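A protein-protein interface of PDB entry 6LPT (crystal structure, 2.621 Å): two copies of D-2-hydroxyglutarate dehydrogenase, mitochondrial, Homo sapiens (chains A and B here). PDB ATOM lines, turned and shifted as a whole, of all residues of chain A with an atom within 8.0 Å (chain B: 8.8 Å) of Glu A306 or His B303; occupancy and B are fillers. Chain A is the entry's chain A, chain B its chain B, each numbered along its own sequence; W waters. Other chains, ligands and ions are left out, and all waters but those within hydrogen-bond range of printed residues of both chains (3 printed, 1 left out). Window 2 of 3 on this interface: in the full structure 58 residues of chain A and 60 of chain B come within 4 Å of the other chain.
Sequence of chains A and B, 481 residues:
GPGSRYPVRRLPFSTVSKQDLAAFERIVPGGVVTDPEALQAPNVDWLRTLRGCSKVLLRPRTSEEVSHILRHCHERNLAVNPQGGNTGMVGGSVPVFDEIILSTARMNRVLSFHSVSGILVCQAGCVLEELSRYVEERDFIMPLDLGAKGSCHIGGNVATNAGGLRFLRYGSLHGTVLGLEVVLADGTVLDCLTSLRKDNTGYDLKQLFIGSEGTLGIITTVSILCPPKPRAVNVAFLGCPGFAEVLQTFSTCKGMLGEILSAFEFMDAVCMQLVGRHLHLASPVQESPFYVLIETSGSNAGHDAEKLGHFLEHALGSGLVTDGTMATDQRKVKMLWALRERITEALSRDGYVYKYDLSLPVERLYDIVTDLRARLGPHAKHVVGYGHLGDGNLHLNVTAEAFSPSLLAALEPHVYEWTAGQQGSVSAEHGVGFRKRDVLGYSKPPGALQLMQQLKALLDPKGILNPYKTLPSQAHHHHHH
Printed residues of chain B within 4 Å of Glu A306: His B303 (3.7 Å).
Of chain A, only His A303, Glu A306 and Lys A307 come within 4 Å of His B303.
Ala A305 touches none of the printed residues of chain B.
No residue of chain A comes within 4 Å of Gly B302.
Of the printed residues of chain A, Ile B260 touches Glu A259.
Of the printed residues of chain A, Ser B299 touches Leu A257 (3.6 Å), Glu A259 (3.0 Å) and Lys A307 (3.3 Å).
Of the printed residues of chain A, Lys B307 touches Asn A300 (3.4 Å) and His A303 (3.3 Å).
Asp B304 touches none of the printed residues of chain A.
The nearest residue of chain B that does not touch Glu A306 is Glu B306 (5.7 Å).
The nearest residue of chain A that does not touch His B303 is Gly A302 (5.6 Å).
Among the printed residues, pairs that only touch across the chains: Leu A257 with Ser B299 (3.6 Å), Glu A259 with Glu B259 (3.7 Å), Glu A259 with Ile B260 (3.8 Å), Glu A259 with Gly B298 (3.6 Å), Asn A300 with Lys B307 (3.4 Å), His A303 with His B303 (3.3 Å), Glu A306 with His B303 (3.7 Å), Lys A307 with Ser B299 (3.3 Å) and Lys A307 with Asn B300 (3.8 Å).
Water W1 lies within hydrogen-bond range of the backbone carbonyl oxygen of Met A256 (2.6 Å) and the side-chain hydroxyl of Ser B299 (2.8 Å).
Water W2 lies within hydrogen-bond range of OD1 of Asp A304 (2.7 Å), N of Asn A300 (2.8 Å), OE1 of Glu B259 (2.9 Å) and NZ of Lys B307 (2.9 Å).
Water W3 lies within hydrogen-bond range of the side-chain carboxylate (OE2) of Glu A259 (2.8 Å), the side-chain carboxylate (OE1) of Glu B259 (2.9 Å) and the side-chain amino group (NZ) of Lys A307 (3.3 Å).
OE2 of Glu A259 lies within salt-bridge range of NZ of Lys A307 (3.8 Å).
The backbone NH (N) of His A303 lies within hydrogen-bond range of the side-chain amide oxygen (OD1) of Asn A300 (3.1 Å).
A ring nitrogen (ND1) of His A310 sits at hydrogen-bond distance from the backbone carbonyl oxygen (O) of Glu A306.
The side-chain carboxylate of Glu B259 lies within salt-bridge range of the side-chain amino group of Lys B307 (3.5 Å).
The side-chain amide oxygen (OD1) of Asn B300 is in hydrogen-bond range of the backbone NH (N) of Gly B302 (3.2 Å).
OD1 of Asn B300 sits at hydrogen-bond distance from N of His B303, at 3.1 Å.
Of the 19 printed residues of chain A, 6 touch a printed residue of chain B.
Printed residues of chain A that touch a printed residue of chain B: Leu A257, Glu A259, Asn A300, His A303, Glu A306 and Lys A307.
Among the printed residues, 13 pairs touch across the chains.
Among the printed residues, no Asp or Glu carboxylate lies within 4 Å of a Lys or Arg side-chain nitrogen of the other chain.
Glu A259 touches Ile B260, but with the chains exchanged Ile A260 does not touch Glu B259 (4.001 Å).
His B303 touches its own counterpart, His A303.
His A303 touches Glu B306, and with the chains exchanged Glu A306 touches His B303.
His A303 touches Lys B307, and with the chains exchanged Lys A307 touches His B303.
The backbone NH (N) of Ser B299 lies within hydrogen-bond range of the side-chain carboxylate (OE1) of Glu A259.
A ring nitrogen (NE2) of His A303 sits at hydrogen-bond distance from the side-chain carboxylate of Glu B306 (3.1 Å).
ND1 of His A303 is in hydrogen-bond range of NZ of Lys B307, at 3.3 Å.
A ring nitrogen (ND1) of His B303 lies within hydrogen-bond range of the side-chain amino group of Lys A307 (3.0 Å).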
ATOM      1  N   ASN A 234      20.947 -19.584 -30.894  1.00  0.00           N
ATOM      2  CA  ASN A 234      20.043 -18.704 -31.623  1.00  0.00           C
ATOM      3  C   ASN A 234      20.461 -18.611 -33.081  1.00  0.00           C
ATOM      4  O   ASN A 234      21.648 -18.689 -33.408  1.00  0.00           O
ATOM      5  CB  ASN A 234      19.995 -17.300 -31.004  1.00  0.00           C
ATOM      6  CG  ASN A 234      19.380 -17.297 -29.620  1.00  0.00           C
ATOM      7  OD1 ASN A 234      18.162 -17.191 -29.469  1.00  0.00           O
ATOM      8  ND2 ASN A 234      20.219 -17.417 -28.600  1.00  0.00           N
ATOM      9  N   MET A 256      29.200  -6.680 -31.798  1.00  0.00           N
ATOM     10  CA  MET A 256      28.080  -6.685 -30.863  1.00  0.00           C
ATOM     11  C   MET A 256      27.741  -8.051 -30.283  1.00  0.00           C
ATOM     12  O   MET A 256      27.168  -8.117 -29.189  1.00  0.00           O
ATOM     13  CB  MET A 256      26.836  -6.109 -31.547  1.00  0.00           C
ATOM     14  CG  MET A 256      27.014  -4.669 -32.011  1.00  0.00           C
ATOM     15  SD  MET A 256      25.477  -3.892 -32.555  1.00  0.00           S
ATOM     16  CE  MET A 256      24.675  -3.579 -30.983  1.00  0.00           C
ATOM     17  N   LEU A 257      28.063  -9.142 -30.977  1.00  0.00           N
ATOM     18  CA  LEU A 257      27.836 -10.489 -30.462  1.00  0.00           C
ATOM     19  C   LEU A 257      29.104 -11.125 -29.918  1.00  0.00           C
ATOM     20  O   LEU A 257      29.065 -11.776 -28.868  1.00  0.00           O
ATOM     21  CB  LEU A 257      27.237 -11.388 -31.548  1.00  0.00           C
ATOM     22  CG  LEU A 257      25.915 -10.906 -32.153  1.00  0.00           C
ATOM     23  CD1 LEU A 257      25.387 -11.902 -33.174  1.00  0.00           C
ATOM     24  CD2 LEU A 257      24.879 -10.651 -31.065  1.00  0.00           C
ATOM     25  N   GLU A 259      32.037 -13.193 -28.616  1.00  0.00           N
ATOM     26  CA  GLU A 259      32.393 -14.576 -28.313  1.00  0.00           C
ATOM     27  C   GLU A 259      31.234 -15.563 -28.437  1.00  0.00           C
ATOM     28  O   GLU A 259      31.486 -16.767 -28.548  1.00  0.00           O
ATOM     29  CB  GLU A 259      33.009 -14.681 -26.913  1.00  0.00           C
ATOM     30  CG  GLU A 259      32.071 -14.434 -25.730  1.00  0.00           C
ATOM     31  CD  GLU A 259      31.647 -12.985 -25.580  1.00  0.00           C
ATOM     32  OE1 GLU A 259      32.239 -12.112 -26.248  1.00  0.00           O
ATOM     33  OE2 GLU A 259      30.730 -12.716 -24.777  1.00  0.00           O
ATOM     34  N   ILE A 260      29.979 -15.110 -28.430  1.00  0.00           N
ATOM     35  CA  ILE A 260      28.895 -16.076 -28.605  1.00  0.00           C
ATOM     36  C   ILE A 260      28.668 -16.452 -30.060  1.00  0.00           C
ATOM     37  O   ILE A 260      27.923 -17.402 -30.330  1.00  0.00           O
ATOM     38  CB  ILE A 260      27.576 -15.578 -27.987  1.00  0.00           C
ATOM     39  CG1 ILE A 260      27.028 -14.377 -28.757  1.00  0.00           C
ATOM     40  CG2 ILE A 260      27.764 -15.249 -26.510  1.00  0.00           C
ATOM     41  CD1 ILE A 260      25.600 -14.020 -28.376  1.00  0.00           C
ATOM     42  N   ASN A 300      24.599 -18.555 -21.176  1.00  0.00           N
ATOM     43  CA  ASN A 300      23.512 -17.832 -20.522  1.00  0.00           C
ATOM     44  C   ASN A 300      22.547 -17.361 -21.603  1.00  0.00           C
ATOM     45  O   ASN A 300      22.855 -16.433 -22.360  1.00  0.00           O
ATOM     46  CB  ASN A 300      24.040 -16.663 -19.691  1.00  0.00           C
ATOM     47  CG  ASN A 300      22.953 -15.995 -18.868  1.00  0.00           C
ATOM     48  OD1 ASN A 300      21.890 -15.646 -19.379  1.00  0.00           O
ATOM     49  ND2 ASN A 300      23.215 -15.823 -17.580  1.00  0.00           N
ATOM     50  N   ALA A 301      21.383 -18.012 -21.673  1.00  0.00           N
ATOM     51  CA  ALA A 301      20.415 -17.722 -22.727  1.00  0.00           C
ATOM     52  C   ALA A 301      19.931 -16.277 -22.686  1.00  0.00           C
ATOM     53  O   ALA A 301      19.701 -15.666 -23.736  1.00  0.00           O
ATOM     54  CB  ALA A 301      19.232 -18.682 -22.620  1.00  0.00           C
ATOM     55  N   GLY A 302      19.779 -15.708 -21.489  1.00  0.00           N
ATOM     56  CA  GLY A 302      19.309 -14.334 -21.396  1.00  0.00           C
ATOM     57  C   GLY A 302      20.313 -13.315 -21.897  1.00  0.00           C
ATOM     58  O   GLY A 302      19.951 -12.367 -22.600  1.00  0.00           O
ATOM     59  N   HIS A 303      21.592 -13.504 -21.558  1.00  0.00           N
ATOM     60  CA  HIS A 303      22.628 -12.612 -22.071  1.00  0.00           C
ATOM     61  C   HIS A 303      22.715 -12.691 -23.589  1.00  0.00           C
ATOM     62  O   HIS A 303      22.843 -11.665 -24.268  1.00  0.00           O
ATOM     63  CB  HIS A 303      23.974 -12.951 -21.433  1.00  0.00           C
ATOM     64  CG  HIS A 303      24.045 -12.638 -19.971  1.00  0.00           C
ATOM     65  ND1 HIS A 303      24.826 -13.359 -19.094  1.00  0.00           N
ATOM     66  CD2 HIS A 303      23.430 -11.685 -19.232  1.00  0.00           C
ATOM     67  CE1 HIS A 303      24.690 -12.864 -17.877  1.00  0.00           C
ATOM     68  NE2 HIS A 303      23.848 -11.847 -17.933  1.00  0.00           N
ATOM     69  N   ASP A 304      22.650 -13.906 -24.137  1.00  0.00           N
ATOM     70  CA  ASP A 304      22.652 -14.073 -25.587  1.00  0.00           C
ATOM     71  C   ASP A 304      21.463 -13.369 -26.223  1.00  0.00           C
ATOM     72  O   ASP A 304      21.607 -12.684 -27.240  1.00  0.00           O
ATOM     73  CB  ASP A 304      22.652 -15.556 -25.950  1.00  0.00           C
ATOM     74  CG  ASP A 304      23.923 -16.251 -25.540  1.00  0.00           C
ATOM     75  OD1 ASP A 304      24.764 -15.617 -24.867  1.00  0.00           O
ATOM     76  OD2 ASP A 304      24.086 -17.431 -25.907  1.00  0.00           O
ATOM     77  N   ALA A 305      20.265 -13.591 -25.677  1.00  0.00           N
ATOM     78  CA  ALA A 305      19.069 -12.956 -26.218  1.00  0.00           C
ATOM     79  C   ALA A 305      19.182 -11.436 -26.182  1.00  0.00           C
ATOM     80  O   ALA A 305      18.767 -10.757 -27.127  1.00  0.00           O
ATOM     81  CB  ALA A 305      17.833 -13.420 -25.447  1.00  0.00           C
ATOM     82  N   GLU A 306      19.745 -10.884 -25.106  1.00  0.00           N
ATOM     83  CA  GLU A 306      19.960  -9.440 -25.039  1.00  0.00           C
ATOM     84  C   GLU A 306      20.950  -8.960 -26.100  1.00  0.00           C
ATOM     85  O   GLU A 306      20.723  -7.928 -26.756  1.00  0.00           O
ATOM     86  CB  GLU A 306      20.447  -9.080 -23.638  1.00  0.00           C
ATOM     87  CG  GLU A 306      19.354  -9.170 -22.577  1.00  0.00           C
ATOM     88  CD  GLU A 306      19.824  -8.733 -21.199  1.00  0.00           C
ATOM     89  OE1 GLU A 306      19.839  -9.586 -20.280  1.00  0.00           O
ATOM     90  OE2 GLU A 306      20.188  -7.547 -21.036  1.00  0.00           O
ATOM     91  N   LYS A 307      22.045  -9.702 -26.293  1.00  0.00           N
ATOM     92  CA  LYS A 307      23.010  -9.339 -27.328  1.00  0.00           C
ATOM     93  C   LYS A 307      22.370  -9.353 -28.709  1.00  0.00           C
ATOM     94  O   LYS A 307      22.548  -8.418 -29.500  1.00  0.00           O
ATOM     95  CB  LYS A 307      24.205 -10.291 -27.289  1.00  0.00           C
ATOM     96  CG  LYS A 307      25.218 -10.003 -26.202  1.00  0.00           C
ATOM     97  CD  LYS A 307      26.378 -10.988 -26.281  1.00  0.00           C
ATOM     98  CE  LYS A 307      27.511 -10.594 -25.342  1.00  0.00           C
ATOM     99  NZ  LYS A 307      27.315 -11.147 -23.975  1.00  0.00           N
ATOM    100  N   LEU A 308      21.613 -10.412 -29.011  1.00  0.00           N
ATOM    101  CA  LEU A 308      20.931 -10.497 -30.299  1.00  0.00           C
ATOM    102  C   LEU A 308      19.923  -9.371 -30.460  1.00  0.00           C
ATOM    103  O   LEU A 308      19.790  -8.808 -31.549  1.00  0.00           O
ATOM    104  CB  LEU A 308      20.243 -11.855 -30.467  1.00  0.00           C
ATOM    105  CG  LEU A 308      21.049 -13.016 -31.065  1.00  0.00           C
ATOM    106  CD1 LEU A 308      21.592 -12.633 -32.437  1.00  0.00           C
ATOM    107  CD2 LEU A 308      22.179 -13.464 -30.157  1.00  0.00           C
ATOM    108  N   GLY A 309      19.151  -9.081 -29.412  1.00  0.00           N
ATOM    109  CA  GLY A 309      18.196  -7.989 -29.485  1.00  0.00           C
ATOM    110  C   GLY A 309      18.838  -6.665 -29.855  1.00  0.00           C
ATOM    111  O   GLY A 309      18.386  -5.976 -30.773  1.00  0.00           O
ATOM    112  N   HIS A 310      19.895  -6.284 -29.130  1.00  0.00           N
ATOM    113  CA  HIS A 310      20.561  -5.015 -29.427  1.00  0.00           C
ATOM    114  C   HIS A 310      21.210  -5.026 -30.810  1.00  0.00           C
ATOM    115  O   HIS A 310      21.125  -4.034 -31.554  1.00  0.00           O
ATOM    116  CB  HIS A 310      21.576  -4.693 -28.330  1.00  0.00           C
ATOM    117  CG  HIS A 310      20.943  -4.306 -27.030  1.00  0.00           C
ATOM    118  ND1 HIS A 310      21.250  -4.920 -25.835  1.00  0.00           N
ATOM    119  CD2 HIS A 310      20.005  -3.372 -26.740  1.00  0.00           C
ATOM    120  CE1 HIS A 310      20.534  -4.377 -24.866  1.00  0.00           C
ATOM    121  NE2 HIS A 310      19.771  -3.434 -25.388  1.00  0.00           N
ATOM    122  N   PHE A 311      21.810  -6.155 -31.198  1.00  0.00           N
ATOM    123  CA  PHE A 311      22.386  -6.280 -32.534  1.00  0.00           C
ATOM    124  C   PHE A 311      21.335  -6.090 -33.616  1.00  0.00           C
ATOM    125  O   PHE A 311      21.532  -5.320 -34.563  1.00  0.00           O
ATOM    126  CB  PHE A 311      23.058  -7.640 -32.693  1.00  0.00           C
ATOM    127  CG  PHE A 311      23.453  -7.943 -34.105  1.00  0.00           C
ATOM    128  CD1 PHE A 311      24.482  -7.256 -34.719  1.00  0.00           C
ATOM    129  CD2 PHE A 311      22.764  -8.902 -34.830  1.00  0.00           C
ATOM    130  CE1 PHE A 311      24.823  -7.531 -36.028  1.00  0.00           C
ATOM    131  CE2 PHE A 311      23.103  -9.182 -36.137  1.00  0.00           C
ATOM    132  CZ  PHE A 311      24.136  -8.498 -36.736  1.00  0.00           C
ATOM    133  N   LEU A 312      20.228  -6.822 -33.510  1.00  0.00           N
ATOM    134  CA  LEU A 312      19.156  -6.741 -34.491  1.00  0.00           C
ATOM    135  C   LEU A 312      18.593  -5.330 -34.560  1.00  0.00           C
ATOM    136  O   LEU A 312      18.343  -4.802 -35.650  1.00  0.00           O
ATOM    137  CB  LEU A 312      18.059  -7.745 -34.137  1.00  0.00           C
ATOM    138  CG  LEU A 312      17.223  -8.300 -35.287  1.00  0.00           C
ATOM    139  CD1 LEU A 312      18.041  -9.294 -36.091  1.00  0.00           C
ATOM    140  CD2 LEU A 312      15.945  -8.940 -34.768  1.00  0.00           C
ATOM    141  N   GLU A 313      18.300  -4.739 -33.399  1.00  0.00           N
ATOM    142  CA  GLU A 313      17.783  -3.376 -33.359  1.00  0.00           C
ATOM    143  C   GLU A 313      18.695  -2.413 -34.110  1.00  0.00           C
ATOM    144  O   GLU A 313      18.230  -1.615 -34.931  1.00  0.00           O
ATOM    145  CB  GLU A 313      17.608  -2.927 -31.907  1.00  0.00           C
ATOM    146  N   ALA B 232      36.066  -6.425 -22.464  1.00  0.00           N
ATOM    147  CA  ALA B 232      36.076  -6.553 -21.016  1.00  0.00           C
ATOM    148  C   ALA B 232      36.941  -7.736 -20.617  1.00  0.00           C
ATOM    149  O   ALA B 232      36.762  -8.848 -21.126  1.00  0.00           O
ATOM    150  CB  ALA B 232      34.656  -6.727 -20.463  1.00  0.00           C
ATOM    151  N   ASN B 234      38.218  -9.554 -16.992  1.00  0.00           N
ATOM    152  CA  ASN B 234      38.111  -9.651 -15.547  1.00  0.00           C
ATOM    153  C   ASN B 234      39.091 -10.688 -15.031  1.00  0.00           C
ATOM    154  O   ASN B 234      39.361 -11.687 -15.705  1.00  0.00           O
ATOM    155  CB  ASN B 234      36.696 -10.061 -15.144  1.00  0.00           C
ATOM    156  CG  ASN B 234      35.685  -8.961 -15.354  1.00  0.00           C
ATOM    157  OD1 ASN B 234      35.359  -8.219 -14.434  1.00  0.00           O
ATOM    158  ND2 ASN B 234      35.183  -8.845 -16.578  1.00  0.00           N
ATOM    159  N   MET B 256      29.302 -21.937 -15.285  1.00  0.00           N
ATOM    160  CA  MET B 256      28.673 -20.638 -15.072  1.00  0.00           C
ATOM    161  C   MET B 256      29.284 -19.493 -15.869  1.00  0.00           C
ATOM    162  O   MET B 256      28.573 -18.535 -16.182  1.00  0.00           O
ATOM    163  CB  MET B 256      28.702 -20.289 -13.581  1.00  0.00           C
ATOM    164  CG  MET B 256      27.894 -21.276 -12.753  1.00  0.00           C
ATOM    165  SD  MET B 256      27.762 -20.865 -11.011  1.00  0.00           S
ATOM    166  CE  MET B 256      26.685 -19.449 -11.126  1.00  0.00           C
ATOM    167  N   LEU B 257      30.572 -19.561 -16.207  1.00  0.00           N
ATOM    168  CA  LEU B 257      31.188 -18.534 -17.041  1.00  0.00           C
ATOM    169  C   LEU B 257      31.188 -18.935 -18.508  1.00  0.00           C
ATOM    170  O   LEU B 257      30.993 -18.084 -19.384  1.00  0.00           O
ATOM    171  CB  LEU B 257      32.616 -18.244 -16.571  1.00  0.00           C
ATOM    172  CG  LEU B 257      32.788 -17.918 -15.086  1.00  0.00           C
ATOM    173  CD1 LEU B 257      34.240 -17.608 -14.755  1.00  0.00           C
ATOM    174  CD2 LEU B 257      31.893 -16.750 -14.699  1.00  0.00           C
ATOM    175  N   GLU B 259      31.673 -19.584 -22.224  1.00  0.00           N
ATOM    176  CA  GLU B 259      32.463 -19.081 -23.341  1.00  0.00           C
ATOM    177  C   GLU B 259      33.300 -17.849 -23.005  1.00  0.00           C
ATOM    178  O   GLU B 259      34.252 -17.557 -23.737  1.00  0.00           O
ATOM    179  CB  GLU B 259      31.549 -18.794 -24.538  1.00  0.00           C
ATOM    180  CG  GLU B 259      30.636 -17.584 -24.386  1.00  0.00           C
ATOM    181  CD  GLU B 259      29.455 -17.845 -23.461  1.00  0.00           C
ATOM    182  OE1 GLU B 259      28.822 -16.865 -23.006  1.00  0.00           O
ATOM    183  OE2 GLU B 259      29.155 -19.033 -23.200  1.00  0.00           O
ATOM    184  N   ILE B 260      32.997 -17.117 -21.928  1.00  0.00           N
ATOM    185  CA  ILE B 260      33.841 -15.965 -21.608  1.00  0.00           C
ATOM    186  C   ILE B 260      35.102 -16.333 -20.843  1.00  0.00           C
ATOM    187  O   ILE B 260      35.985 -15.479 -20.693  1.00  0.00           O
ATOM    188  CB  ILE B 260      33.091 -14.877 -20.813  1.00  0.00           C
ATOM    189  CG1 ILE B 260      32.811 -15.330 -19.379  1.00  0.00           C
ATOM    190  CG2 ILE B 260      31.812 -14.478 -21.537  1.00  0.00           C
ATOM    191  CD1 ILE B 260      32.351 -14.208 -18.477  1.00  0.00           C
ATOM    192  N   THR B 296      38.435 -13.869 -17.399  1.00  0.00           N
ATOM    193  CA  THR B 296      37.395 -13.849 -18.413  1.00  0.00           C
ATOM    194  C   THR B 296      37.618 -12.715 -19.401  1.00  0.00           C
ATOM    195  O   THR B 296      38.129 -11.646 -19.048  1.00  0.00           O
ATOM    196  CB  THR B 296      36.006 -13.676 -17.785  1.00  0.00           C
ATOM    197  OG1 THR B 296      35.934 -12.406 -17.126  1.00  0.00           O
ATOM    198  CG2 THR B 296      35.730 -14.773 -16.777  1.00  0.00           C
ATOM    199  N   GLY B 298      35.395 -10.883 -22.690  1.00  0.00           N
ATOM    200  CA  GLY B 298      34.143 -10.861 -23.423  1.00  0.00           C
ATOM    201  C   GLY B 298      33.815  -9.507 -24.007  1.00  0.00           C
ATOM    202  O   GLY B 298      34.501  -8.508 -23.771  1.00  0.00           O
ATOM    203  N   SER B 299      32.727  -9.499 -24.783  1.00  0.00           N
ATOM    204  CA  SER B 299      32.310  -8.314 -25.522  1.00  0.00           C
ATOM    205  C   SER B 299      31.461  -7.366 -24.686  1.00  0.00           C
ATOM    206  O   SER B 299      31.453  -6.161 -24.959  1.00  0.00           O
ATOM    207  CB  SER B 299      31.556  -8.721 -26.791  1.00  0.00           C
ATOM    208  OG  SER B 299      30.361  -9.410 -26.477  1.00  0.00           O
ATOM    209  N   ASN B 300      30.748  -7.873 -23.678  1.00  0.00           N
ATOM    210  CA  ASN B 300      29.808  -7.067 -22.903  1.00  0.00           C
ATOM    211  C   ASN B 300      30.200  -7.111 -21.429  1.00  0.00           C
ATOM    212  O   ASN B 300      30.065  -8.149 -20.769  1.00  0.00           O
ATOM    213  CB  ASN B 300      28.373  -7.555 -23.100  1.00  0.00           C
ATOM    214  CG  ASN B 300      27.344  -6.539 -22.641  1.00  0.00           C
ATOM    215  OD1 ASN B 300      27.180  -6.303 -21.444  1.00  0.00           O
ATOM    216  ND2 ASN B 300      26.640  -5.940 -23.593  1.00  0.00           N
ATOM    217  N   ALA B 301      30.694  -5.975 -20.930  1.00  0.00           N
ATOM    218  CA  ALA B 301      31.112  -5.852 -19.536  1.00  0.00           C
ATOM    219  C   ALA B 301      30.004  -6.243 -18.560  1.00  0.00           C
ATOM    220  O   ALA B 301      30.227  -7.033 -17.639  1.00  0.00           O
ATOM    221  CB  ALA B 301      31.585  -4.422 -19.265  1.00  0.00           C
ATOM    222  N   GLY B 302      28.818  -5.647 -18.719  1.00  0.00           N
ATOM    223  CA  GLY B 302      27.684  -5.983 -17.863  1.00  0.00           C
ATOM    224  C   GLY B 302      27.376  -7.467 -17.777  1.00  0.00           C
ATOM    225  O   GLY B 302      27.194  -8.016 -16.684  1.00  0.00           O
ATOM    226  N   HIS B 303      27.336  -8.146 -18.926  1.00  0.00           N
ATOM    227  CA  HIS B 303      27.039  -9.575 -18.924  1.00  0.00           C
ATOM    228  C   HIS B 303      28.146 -10.378 -18.246  1.00  0.00           C
ATOM    229  O   HIS B 303      27.861 -11.304 -17.474  1.00  0.00           O
ATOM    230  CB  HIS B 303      26.815 -10.066 -20.356  1.00  0.00           C
ATOM    231  CG  HIS B 303      25.635  -9.441 -21.038  1.00  0.00           C
ATOM    232  ND1 HIS B 303      25.518  -9.376 -22.409  1.00  0.00           N
ATOM    233  CD2 HIS B 303      24.524  -8.846 -20.540  1.00  0.00           C
ATOM    234  CE1 HIS B 303      24.387  -8.773 -22.728  1.00  0.00           C
ATOM    235  NE2 HIS B 303      23.764  -8.442 -21.611  1.00  0.00           N
ATOM    236  N   ASP B 304      29.410 -10.054 -18.533  1.00  0.00           N
ATOM    237  CA  ASP B 304      30.518 -10.762 -17.897  1.00  0.00           C
ATOM    238  C   ASP B 304      30.504 -10.557 -16.388  1.00  0.00           C
ATOM    239  O   ASP B 304      30.782 -11.486 -15.619  1.00  0.00           O
ATOM    240  CB  ASP B 304      31.845 -10.293 -18.487  1.00  0.00           C
ATOM    241  CG  ASP B 304      32.003 -10.680 -19.938  1.00  0.00           C
ATOM    242  OD1 ASP B 304      31.024 -11.173 -20.536  1.00  0.00           O
ATOM    243  OD2 ASP B 304      33.112 -10.495 -20.479  1.00  0.00           O
ATOM    244  N   ALA B 305      30.188  -9.335 -15.951  1.00  0.00           N
ATOM    245  CA  ALA B 305      30.075  -9.045 -14.527  1.00  0.00           C
ATOM    246  C   ALA B 305      28.965  -9.859 -13.882  1.00  0.00           C
ATOM    247  O   ALA B 305      29.135 -10.378 -12.777  1.00  0.00           O
ATOM    248  CB  ALA B 305      29.835  -7.550 -14.313  1.00  0.00           C
ATOM    249  N   GLU B 306      27.813  -9.965 -14.546  1.00  0.00           N
ATOM    250  CA  GLU B 306      26.732 -10.794 -14.018  1.00  0.00           C
ATOM    251  C   GLU B 306      27.144 -12.263 -13.906  1.00  0.00           C
ATOM    252  O   GLU B 306      26.903 -12.911 -12.875  1.00  0.00           O
ATOM    253  CB  GLU B 306      25.493 -10.643 -14.897  1.00  0.00           C
ATOM    254  CG  GLU B 306      24.436  -9.724 -14.314  1.00  0.00           C
ATOM    255  CD  GLU B 306      23.196  -9.632 -15.181  1.00  0.00           C
ATOM    256  OE1 GLU B 306      22.558 -10.681 -15.424  1.00  0.00           O
ATOM    257  OE2 GLU B 306      22.859  -8.507 -15.611  1.00  0.00           O
ATOM    258  N   LYS B 307      27.759 -12.809 -14.961  1.00  0.00           N
ATOM    259  CA  LYS B 307      28.253 -14.186 -14.901  1.00  0.00           C
ATOM    260  C   LYS B 307      29.218 -14.390 -13.739  1.00  0.00           C
ATOM    261  O   LYS B 307      29.084 -15.348 -12.970  1.00  0.00           O
ATOM    262  CB  LYS B 307      28.936 -14.583 -16.213  1.00  0.00           C
ATOM    263  CG  LYS B 307      28.009 -14.970 -17.353  1.00  0.00           C
ATOM    264  CD  LYS B 307      28.815 -15.572 -18.500  1.00  0.00           C
ATOM    265  CE  LYS B 307      28.444 -14.969 -19.845  1.00  0.00           C
ATOM    266  NZ  LYS B 307      27.113 -15.430 -20.321  1.00  0.00           N
ATOM    267  N   LEU B 308      30.204 -13.500 -13.601  1.00  0.00           N
ATOM    268  CA  LEU B 308      31.172 -13.637 -12.517  1.00  0.00           C
ATOM    269  C   LEU B 308      30.518 -13.496 -11.151  1.00  0.00           C
ATOM    270  O   LEU B 308      30.863 -14.228 -10.220  1.00  0.00           O
ATOM    271  CB  LEU B 308      32.297 -12.623 -12.683  1.00  0.00           C
ATOM    272  CG  LEU B 308      33.397 -13.151 -13.600  1.00  0.00           C
ATOM    273  CD1 LEU B 308      34.078 -12.009 -14.297  1.00  0.00           C
ATOM    274  CD2 LEU B 308      34.396 -13.975 -12.807  1.00  0.00           C
ATOM    275  N   GLY B 309      29.629 -12.517 -10.987  1.00  0.00           N
ATOM    276  CA  GLY B 309      28.932 -12.367  -9.722  1.00  0.00           C
ATOM    277  C   GLY B 309      28.186 -13.620  -9.309  1.00  0.00           C
ATOM    278  O   GLY B 309      28.298 -14.076  -8.168  1.00  0.00           O
ATOM    279  N   HIS B 310      27.421 -14.206 -10.237  1.00  0.00           N
ATOM    280  CA  HIS B 310      26.697 -15.433  -9.907  1.00  0.00           C
ATOM    281  C   HIS B 310      27.659 -16.592  -9.643  1.00  0.00           C
ATOM    282  O   HIS B 310      27.438 -17.392  -8.722  1.00  0.00           O
ATOM    283  CB  HIS B 310      25.700 -15.768 -11.018  1.00  0.00           C
ATOM    284  CG  HIS B 310      24.647 -16.756 -10.613  1.00  0.00           C
ATOM    285  ND1 HIS B 310      24.252 -16.922  -9.303  1.00  0.00           N
ATOM    286  CD2 HIS B 310      23.871 -17.588 -11.347  1.00  0.00           C
ATOM    287  CE1 HIS B 310      23.301 -17.838  -9.244  1.00  0.00           C
ATOM    288  NE2 HIS B 310      23.050 -18.257 -10.471  1.00  0.00           N
HETATM  289  O   HOH W   1      28.215  -7.607 -26.861  1.00  0.00           O
HETATM  290  O   HOH W   2      25.997 -16.629 -22.671  1.00  0.00           O
HETATM  291  O   HOH W   3      28.800 -14.018 -23.192  1.00  0.00           O
